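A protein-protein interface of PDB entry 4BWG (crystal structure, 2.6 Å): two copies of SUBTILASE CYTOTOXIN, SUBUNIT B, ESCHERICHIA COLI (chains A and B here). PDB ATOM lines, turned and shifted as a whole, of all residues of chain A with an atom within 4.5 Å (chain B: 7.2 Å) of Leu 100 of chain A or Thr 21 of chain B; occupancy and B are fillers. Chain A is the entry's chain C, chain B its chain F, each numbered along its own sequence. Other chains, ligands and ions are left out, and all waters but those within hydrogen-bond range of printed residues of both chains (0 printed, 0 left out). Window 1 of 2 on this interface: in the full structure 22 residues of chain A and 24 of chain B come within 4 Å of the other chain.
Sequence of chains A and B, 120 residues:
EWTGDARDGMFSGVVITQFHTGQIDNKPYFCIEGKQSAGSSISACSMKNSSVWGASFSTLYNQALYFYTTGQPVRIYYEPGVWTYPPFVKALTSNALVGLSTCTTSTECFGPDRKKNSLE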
ATOM      1  N   ILE A  16      29.908  12.770  31.863  1.00  0.00           N
ATOM      2  CA  ILE A  16      31.281  12.887  31.334  1.00  0.00           C
ATOM      3  C   ILE A  16      32.193  12.042  32.238  1.00  0.00           C
ATOM      4  O   ILE A  16      32.351  12.348  33.405  1.00  0.00           O
ATOM      5  CB  ILE A  16      31.793  14.341  31.176  1.00  0.00           C
ATOM      6  CG1 ILE A  16      30.898  15.133  30.214  1.00  0.00           C
ATOM      7  CG2 ILE A  16      33.323  14.385  30.756  1.00  0.00           C
ATOM      8  CD1 ILE A  16      31.163  16.656  30.208  1.00  0.00           C
ATOM      9  N   THR A  59      35.582  28.258  26.799  1.00  0.00           N
ATOM     10  CA  THR A  59      34.273  28.101  27.410  1.00  0.00           C
ATOM     11  C   THR A  59      33.957  26.610  27.581  1.00  0.00           C
ATOM     12  O   THR A  59      33.536  26.189  28.667  1.00  0.00           O
ATOM     13  CB  THR A  59      33.200  28.801  26.570  1.00  0.00           C
ATOM     14  OG1 THR A  59      33.565  30.165  26.366  1.00  0.00           O
ATOM     15  CG2 THR A  59      31.825  28.746  27.228  1.00  0.00           C
ATOM     16  N   LEU A  60      34.152  25.823  26.505  1.00  0.00           N
ATOM     17  CA  LEU A  60      33.890  24.378  26.520  1.00  0.00           C
ATOM     18  C   LEU A  60      34.809  23.658  27.503  1.00  0.00           C
ATOM     19  O   LEU A  60      34.337  22.805  28.227  1.00  0.00           O
ATOM     20  CB  LEU A  60      34.027  23.761  25.139  1.00  0.00           C
ATOM     21  CG  LEU A  60      32.971  24.152  24.101  1.00  0.00           C
ATOM     22  CD1 LEU A  60      33.351  23.634  22.770  1.00  0.00           C
ATOM     23  CD2 LEU A  60      31.589  23.654  24.484  1.00  0.00           C
ATOM     24  N   GLN A  63      33.532  24.501  31.107  1.00  0.00           N
ATOM     25  CA  GLN A  63      32.231  23.862  31.283  1.00  0.00           C
ATOM     26  C   GLN A  63      32.343  22.330  31.362  1.00  0.00           C
ATOM     27  O   GLN A  63      31.762  21.742  32.268  1.00  0.00           O
ATOM     28  CB  GLN A  63      31.271  24.275  30.152  1.00  0.00           C
ATOM     29  CG  GLN A  63      29.807  24.204  30.543  1.00  0.00           C
ATOM     30  CD  GLN A  63      29.483  25.074  31.750  1.00  0.00           C
ATOM     31  OE1 GLN A  63      29.548  26.309  31.694  1.00  0.00           O
ATOM     32  NE2 GLN A  63      29.153  24.463  32.876  1.00  0.00           N
ATOM     33  N   ALA A  64      33.085  21.690  30.425  1.00  0.00           N
ATOM     34  CA  ALA A  64      33.325  20.242  30.407  1.00  0.00           C
ATOM     35  C   ALA A  64      34.057  19.772  31.656  1.00  0.00           C
ATOM     36  O   ALA A  64      33.704  18.730  32.192  1.00  0.00           O
ATOM     37  CB  ALA A  64      34.112  19.839  29.165  1.00  0.00           C
ATOM     38  N   PHE A  67      31.438  19.828  34.501  1.00  0.00           N
ATOM     39  CA  PHE A  67      30.482  18.725  34.398  1.00  0.00           C
ATOM     40  C   PHE A  67      31.139  17.366  34.651  1.00  0.00           C
ATOM     41  O   PHE A  67      30.468  16.455  35.171  1.00  0.00           O
ATOM     42  CB  PHE A  67      29.832  18.752  33.030  1.00  0.00           C
ATOM     43  CG  PHE A  67      28.829  19.860  32.843  1.00  0.00           C
ATOM     44  CD1 PHE A  67      28.063  20.335  33.923  1.00  0.00           C
ATOM     45  CD2 PHE A  67      28.553  20.355  31.576  1.00  0.00           C
ATOM     46  CE1 PHE A  67      27.066  21.316  33.721  1.00  0.00           C
ATOM     47  CE2 PHE A  67      27.556  21.328  31.381  1.00  0.00           C
ATOM     48  CZ  PHE A  67      26.817  21.798  32.447  1.00  0.00           C
ATOM     49  N   ARG A  75      23.966  16.994  28.033  1.00  0.00           N
ATOM     50  CA  ARG A  75      23.867  16.787  26.604  1.00  0.00           C
ATOM     51  C   ARG A  75      25.182  17.246  25.998  1.00  0.00           C
ATOM     52  O   ARG A  75      25.648  18.346  26.311  1.00  0.00           O
ATOM     53  CB  ARG A  75      22.703  17.595  26.004  1.00  0.00           C
ATOM     54  CG  ARG A  75      22.639  17.556  24.499  1.00  0.00           C
ATOM     55  CD  ARG A  75      21.369  18.201  24.049  1.00  0.00           C
ATOM     56  NE  ARG A  75      20.169  17.404  24.326  1.00  0.00           N
ATOM     57  CZ  ARG A  75      18.926  17.857  24.160  1.00  0.00           C
ATOM     58  NH1 ARG A  75      18.715  19.102  23.745  1.00  0.00           N
ATOM     59  NH2 ARG A  75      17.886  17.071  24.415  1.00  0.00           N
ATOM     60  N   ILE A  76      25.780  16.399  25.183  1.00  0.00           N
ATOM     61  CA  ILE A  76      26.993  16.687  24.432  1.00  0.00           C
ATOM     62  C   ILE A  76      26.577  16.920  22.988  1.00  0.00           C
ATOM     63  O   ILE A  76      25.943  16.049  22.374  1.00  0.00           O
ATOM     64  CB  ILE A  76      28.056  15.540  24.544  1.00  0.00           C
ATOM     65  CG1 ILE A  76      28.759  15.553  25.903  1.00  0.00           C
ATOM     66  CG2 ILE A  76      29.103  15.611  23.408  1.00  0.00           C
ATOM     67  CD1 ILE A  76      29.398  14.271  26.265  1.00  0.00           C
ATOM     68  N   TYR A  77      26.924  18.097  22.461  1.00  0.00           N
ATOM     69  CA  TYR A  77      26.744  18.475  21.058  1.00  0.00           C
ATOM     70  C   TYR A  77      28.067  18.280  20.341  1.00  0.00           C
ATOM     71  O   TYR A  77      29.099  18.764  20.806  1.00  0.00           O
ATOM     72  CB  TYR A  77      26.312  19.929  20.922  1.00  0.00           C
ATOM     73  CG  TYR A  77      24.973  20.265  21.521  1.00  0.00           C
ATOM     74  CD1 TYR A  77      24.861  20.635  22.854  1.00  0.00           C
ATOM     75  CD2 TYR A  77      23.825  20.305  20.731  1.00  0.00           C
ATOM     76  CE1 TYR A  77      23.640  21.012  23.398  1.00  0.00           C
ATOM     77  CE2 TYR A  77      22.591  20.664  21.269  1.00  0.00           C
ATOM     78  CZ  TYR A  77      22.507  21.031  22.602  1.00  0.00           C
ATOM     79  OH  TYR A  77      21.297  21.400  23.141  1.00  0.00           O
ATOM     80  N   LEU A  97      33.698  18.867  19.723  1.00  0.00           N
ATOM     81  CA  LEU A  97      32.755  19.258  20.746  1.00  0.00           C
ATOM     82  C   LEU A  97      32.303  20.677  20.377  1.00  0.00           C
ATOM     83  O   LEU A  97      33.146  21.561  20.124  1.00  0.00           O
ATOM     84  CB  LEU A  97      33.397  19.218  22.125  1.00  0.00           C
ATOM     85  CG  LEU A  97      32.533  19.634  23.297  1.00  0.00           C
ATOM     86  CD1 LEU A  97      31.290  18.744  23.427  1.00  0.00           C
ATOM     87  CD2 LEU A  97      33.362  19.669  24.572  1.00  0.00           C
ATOM     88  N   GLY A  99      29.166  22.062  21.877  1.00  0.00           N
ATOM     89  CA  GLY A  99      28.223  22.566  22.867  1.00  0.00           C
ATOM     90  C   GLY A  99      27.940  21.616  24.006  1.00  0.00           C
ATOM     91  O   GLY A  99      28.245  20.427  23.914  1.00  0.00           O
ATOM     92  N   LEU A 100      27.341  22.135  25.080  1.00  0.00           N
ATOM     93  CA  LEU A 100      27.006  21.392  26.307  1.00  0.00           C
ATOM     94  C   LEU A 100      25.760  21.971  26.933  1.00  0.00           C
ATOM     95  O   LEU A 100      25.558  23.195  26.876  1.00  0.00           O
ATOM     96  CB  LEU A 100      28.150  21.459  27.344  1.00  0.00           C
ATOM     97  CG  LEU A 100      29.494  20.775  27.010  1.00  0.00           C
ATOM     98  CD1 LEU A 100      30.632  21.360  27.841  1.00  0.00           C
ATOM     99  CD2 LEU A 100      29.396  19.242  27.110  1.00  0.00           C
ATOM    100  N   SER A 101      24.946  21.111  27.559  1.00  0.00           N
ATOM    101  CA  SER A 101      23.737  21.527  28.249  1.00  0.00           C
ATOM    102  C   SER A 101      23.489  20.701  29.446  1.00  0.00           C
ATOM    103  O   SER A 101      23.815  19.520  29.450  1.00  0.00           O
ATOM    104  CB  SER A 101      22.522  21.389  27.339  1.00  0.00           C
ATOM    105  OG  SER A 101      22.506  22.376  26.323  1.00  0.00           O
ATOM    106  N   PHE B  19      21.671  25.473  32.244  1.00  0.00           N
ATOM    107  CA  PHE B  19      22.853  26.099  31.676  1.00  0.00           C
ATOM    108  C   PHE B  19      23.184  25.438  30.358  1.00  0.00           C
ATOM    109  O   PHE B  19      23.186  24.213  30.275  1.00  0.00           O
ATOM    110  CB  PHE B  19      24.061  25.971  32.662  1.00  0.00           C
ATOM    111  CG  PHE B  19      25.049  27.121  32.650  1.00  0.00           C
ATOM    112  CD1 PHE B  19      25.971  27.263  31.608  1.00  0.00           C
ATOM    113  CD2 PHE B  19      25.044  28.082  33.663  1.00  0.00           C
ATOM    114  CE1 PHE B  19      26.879  28.321  31.591  1.00  0.00           C
ATOM    115  CE2 PHE B  19      25.953  29.148  33.636  1.00  0.00           C
ATOM    116  CZ  PHE B  19      26.869  29.252  32.604  1.00  0.00           C
ATOM    117  N   HIS B  20      23.467  26.236  29.330  1.00  0.00           N
ATOM    118  CA  HIS B  20      23.836  25.761  28.001  1.00  0.00           C
ATOM    119  C   HIS B  20      24.949  26.633  27.459  1.00  0.00           C
ATOM    120  O   HIS B  20      24.932  27.826  27.675  1.00  0.00           O
ATOM    121  CB  HIS B  20      22.606  25.765  27.045  1.00  0.00           C
ATOM    122  CG  HIS B  20      22.940  25.657  25.578  1.00  0.00           C
ATOM    123  ND1 HIS B  20      23.468  24.496  25.040  1.00  0.00           N
ATOM    124  CD2 HIS B  20      22.851  26.584  24.600  1.00  0.00           C
ATOM    125  CE1 HIS B  20      23.691  24.753  23.762  1.00  0.00           C
ATOM    126  NE2 HIS B  20      23.334  25.995  23.451  1.00  0.00           N
ATOM    127  N   THR B  21      25.931  26.042  26.796  1.00  0.00           N
ATOM    128  CA  THR B  21      27.021  26.786  26.147  1.00  0.00           C
ATOM    129  C   THR B  21      27.193  26.258  24.733  1.00  0.00           C
ATOM    130  O   THR B  21      27.157  25.053  24.526  1.00  0.00           O
ATOM    131  CB  THR B  21      28.371  26.727  26.935  1.00  0.00           C
ATOM    132  OG1 THR B  21      28.872  25.402  26.935  1.00  0.00           O
ATOM    133  CG2 THR B  21      28.253  27.189  28.352  1.00  0.00           C
ATOM    134  N   GLY B  22      27.406  27.154  23.786  1.00  0.00           N
ATOM    135  CA  GLY B  22      27.649  26.776  22.402  1.00  0.00           C
ATOM    136  C   GLY B  22      28.401  27.855  21.663  1.00  0.00           C
ATOM    137  O   GLY B  22      29.028  28.718  22.286  1.00  0.00           O
ATOM    138  N   GLN B  23      28.307  27.832  20.328  1.00  0.00           N
ATOM    139  CA  GLN B  23      28.927  28.799  19.436  1.00  0.00           C
ATOM    140  C   GLN B  23      28.002  29.071  18.263  1.00  0.00           C
ATOM    141  O   GLN B  23      27.350  28.148  17.760  1.00  0.00           O
ATOM    142  CB  GLN B  23      30.286  28.281  18.935  1.00  0.00           C
ATOM    143  CG  GLN B  23      31.078  29.304  18.124  1.00  0.00           C
ATOM    144  CD  GLN B  23      32.371  28.752  17.614  1.00  0.00           C
ATOM    145  OE1 GLN B  23      33.208  28.267  18.375  1.00  0.00           O
ATOM    146  NE2 GLN B  23      32.576  28.852  16.313  1.00  0.00           N
ATOM    147  N   PRO B  28      31.429  32.387  20.844  1.00  0.00           N
ATOM    148  CA  PRO B  28      30.880  31.532  21.906  1.00  0.00           C
ATOM    149  C   PRO B  28      29.771  32.264  22.650  1.00  0.00           C
ATOM    150  O   PRO B  28      29.782  33.486  22.726  1.00  0.00           O
ATOM    151  CB  PRO B  28      32.089  31.264  22.813  1.00  0.00           C
ATOM    152  CG  PRO B  28      33.001  32.384  22.562  1.00  0.00           C
ATOM    153  CD  PRO B  28      32.793  32.849  21.174  1.00  0.00           C
ATOM    154  N   TYR B  29      28.803  31.526  23.161  1.00  0.00           N
ATOM    155  CA  TYR B  29      27.696  32.090  23.956  1.00  0.00           C
ATOM    156  C   TYR B  29      27.314  31.134  25.081  1.00  0.00           C
ATOM    157  O   TYR B  29      27.671  29.959  25.038  1.00  0.00           O
ATOM    158  CB  TYR B  29      26.444  32.408  23.078  1.00  0.00           C
ATOM    159  CG  TYR B  29      25.736  31.174  22.555  1.00  0.00           C
ATOM    160  CD1 TYR B  29      26.124  30.577  21.356  1.00  0.00           C
ATOM    161  CD2 TYR B  29      24.740  30.548  23.300  1.00  0.00           C
ATOM    162  CE1 TYR B  29      25.518  29.404  20.900  1.00  0.00           C
ATOM    163  CE2 TYR B  29      24.151  29.359  22.869  1.00  0.00           C
ATOM    164  CZ  TYR B  29      24.535  28.798  21.660  1.00  0.00           C
ATOM    165  OH  TYR B  29      23.963  27.639  21.196  1.00  0.00           O
ATOM    166  N   PHE B  30      26.531  31.602  26.029  1.00  0.00           N
ATOM    167  CA  PHE B  30      26.005  30.723  27.071  1.00  0.00           C
ATOM    168  C   PHE B  30      24.595  31.196  27.385  1.00  0.00           C
ATOM    169  O   PHE B  30      24.324  32.411  27.329  1.00  0.00           O
ATOM    170  CB  PHE B  30      26.901  30.627  28.328  1.00  0.00           C
ATOM    171  CG  PHE B  30      26.835  31.824  29.235  1.00  0.00           C
ATOM    172  CD1 PHE B  30      27.623  32.940  28.995  1.00  0.00           C
ATOM    173  CD2 PHE B  30      25.926  31.866  30.293  1.00  0.00           C
ATOM    174  CE1 PHE B  30      27.541  34.056  29.825  1.00  0.00           C
ATOM    175  CE2 PHE B  30      25.812  32.998  31.089  1.00  0.00           C
ATOM    176  CZ  PHE B  30      26.613  34.089  30.843  1.00  0.00           C
ATOM    177  N   CYS B  31      23.710  30.245  27.723  1.00  0.00           N
ATOM    178  CA  CYS B  31      22.304  30.475  28.022  1.00  0.00           C
ATOM    179  C   CYS B  31      21.956  29.926  29.397  1.00  0.00           C
ATOM    180  O   CYS B  31      22.377  28.819  29.741  1.00  0.00           O
ATOM    181  CB  CYS B  31      21.435  29.838  26.941  1.00  0.00           C
ATOM    182  SG  CYS B  31      19.776  30.546  26.800  1.00  0.00           S
ATOM    183  N   PHE B  57      30.626  39.310  28.606  1.00  0.00           N
ATOM    184  CA  PHE B  57      30.516  37.857  28.430  1.00  0.00           C
ATOM    185  C   PHE B  57      31.277  37.062  29.506  1.00  0.00           C
ATOM    186  O   PHE B  57      30.680  36.195  30.134  1.00  0.00           O
ATOM    187  CB  PHE B  57      30.986  37.425  27.019  1.00  0.00           C
ATOM    188  CG  PHE B  57      31.067  35.926  26.829  1.00  0.00           C
ATOM    189  CD1 PHE B  57      29.912  35.170  26.606  1.00  0.00           C
ATOM    190  CD2 PHE B  57      32.285  35.260  26.930  1.00  0.00           C
ATOM    191  CE1 PHE B  57      29.979  33.786  26.471  1.00  0.00           C
ATOM    192  CE2 PHE B  57      32.348  33.867  26.813  1.00  0.00           C
ATOM    193  CZ  PHE B  57      31.193  33.143  26.579  1.00  0.00           C
ATOM    194  N   TYR B  61      29.600  35.038  32.465  1.00  0.00           N
ATOM    195  CA  TYR B  61      29.742  33.588  32.413  1.00  0.00           C
ATOM    196  C   TYR B  61      30.184  33.069  33.767  1.00  0.00           C
ATOM    197  O   TYR B  61      29.582  32.135  34.300  1.00  0.00           O
ATOM    198  CB  TYR B  61      30.714  33.150  31.300  1.00  0.00           C
ATOM    199  CG  TYR B  61      31.035  31.677  31.335  1.00  0.00           C
ATOM    200  CD1 TYR B  61      30.157  30.738  30.800  1.00  0.00           C
ATOM    201  CD2 TYR B  61      32.172  31.208  31.988  1.00  0.00           C
ATOM    202  CE1 TYR B  61      30.427  29.368  30.868  1.00  0.00           C
ATOM    203  CE2 TYR B  61      32.442  29.840  32.085  1.00  0.00           C
ATOM    204  CZ  TYR B  61      31.583  28.926  31.492  1.00  0.00           C
ATOM    205  OH  TYR B  61      31.874  27.586  31.543  1.00  0.00           O
ATOM    206  N   LEU B  92      16.311  28.507  21.733  1.00  0.00           N
ATOM    207  CA  LEU B  92      16.745  29.113  22.990  1.00  0.00           C
ATOM    208  C   LEU B  92      15.873  30.330  23.238  1.00  0.00           C
ATOM    209  O   LEU B  92      14.679  30.146  23.491  1.00  0.00           O
ATOM    210  CB  LEU B  92      18.261  29.445  22.977  1.00  0.00           C
ATOM    211  CG  LEU B  92      19.196  28.238  22.931  1.00  0.00           C
ATOM    212  CD1 LEU B  92      20.478  28.566  22.234  1.00  0.00           C
ATOM    213  CD2 LEU B  92      19.459  27.706  24.300  1.00  0.00           C
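No position is printed for both chains.
The backbone carbonyl oxygen of Ser 101 of chain A is in hydrogen-bond range of the backbone NH of Arg 75 of chain A, at 2.9 Å. N of Tyr 77 of chain A sits at hydrogen-bond distance from O of Gly 99 of chain A, at 3.0 Å. NE2 of His 20 of chain B is in hydrogen-bond range of OH of Tyr 29 of chain B, 2.9 Å away. The backbone NH of Cys 31 of chain B lies within hydrogen-bond range of the backbone carbonyl oxygen of His 20 of chain B (2.7 Å).
Hydrophobic or aromatic side chains of chain A that line the printed part of chain B: Tyr 77. Of the 12 printed residues of chain B, 5 touch a printed residue of chain A.
Among the printed residues, pairs that only touch across the chains: Thr 59 of chain A with Phe 57 of chain B, Thr 59 of chain A with Tyr 61 of chain B, Gln 63 of chain A with Phe 19 of chain B, Gln 63 of chain A with Thr 21 of chain B, Tyr 77 of chain A with His 20 of chain B, Gly 99 of chain A with Thr 21 of chain B and Ser 101 of chain A with Phe 19 of chain B.
Printed residues of chain B within 4 Å of Leu 100 of chain A: His 20 (3.1 Å) and Thr 21 (2.9 Å). Printed residues of chain A within 4 Å of Thr 21 of chain B: Gln 63, Gly 99 and Leu 100. Of the printed residues of chain B, Tyr 77 of chain A touches His 20. Of the printed residues of chain A, Phe 19 of chain B touches Gln 63 and Ser 101. Printed residues of chain B within 4 Å of Thr 59 of chain A: Phe 57 (3.8 Å) and Tyr 61 (3.6 Å). Of the printed residues of chain B, Ser 101 of chain A touches Phe 19 and His 20. Of the printed residues of chain B, Gln 63 of chain A touches Phe 19, Thr 21 and Tyr 61. Phe 67 of chain A touches none of the printed residues of chain B. Leu 60 of chain A touches none of the printed residues of chain B. The nearest residue of chain B that does not touch Leu 100 of chain A is Phe 19 of chain B (4.3 Å). The nearest printed residue of chain A that does not touch Thr 21 of chain B is Thr 59 of chain A (4.01 Å). The nearest printed residue of chain B that does not touch Gln 63 of chain A is Phe 30 of chain B (6.1 Å).
The side-chain hydroxyl (OH) of Tyr 61 of chain B sits at hydrogen-bond distance from the side-chain amide oxygen (OE1) of Gln 63 of chain A, at 2.7 Å. ND1 of His 20 of chain B is in hydrogen-bond range of O of Leu 100 of chain A (3.1 Å). The backbone carbonyl oxygen of Leu 100 of chain A sits at hydrogen-bond distance from the backbone NH of Thr 21 of chain B, 2.9 Å away. OG of Ser 101 of chain A sits at hydrogen-bond distance from ND1 of His 20 of chain B (2.7 Å).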
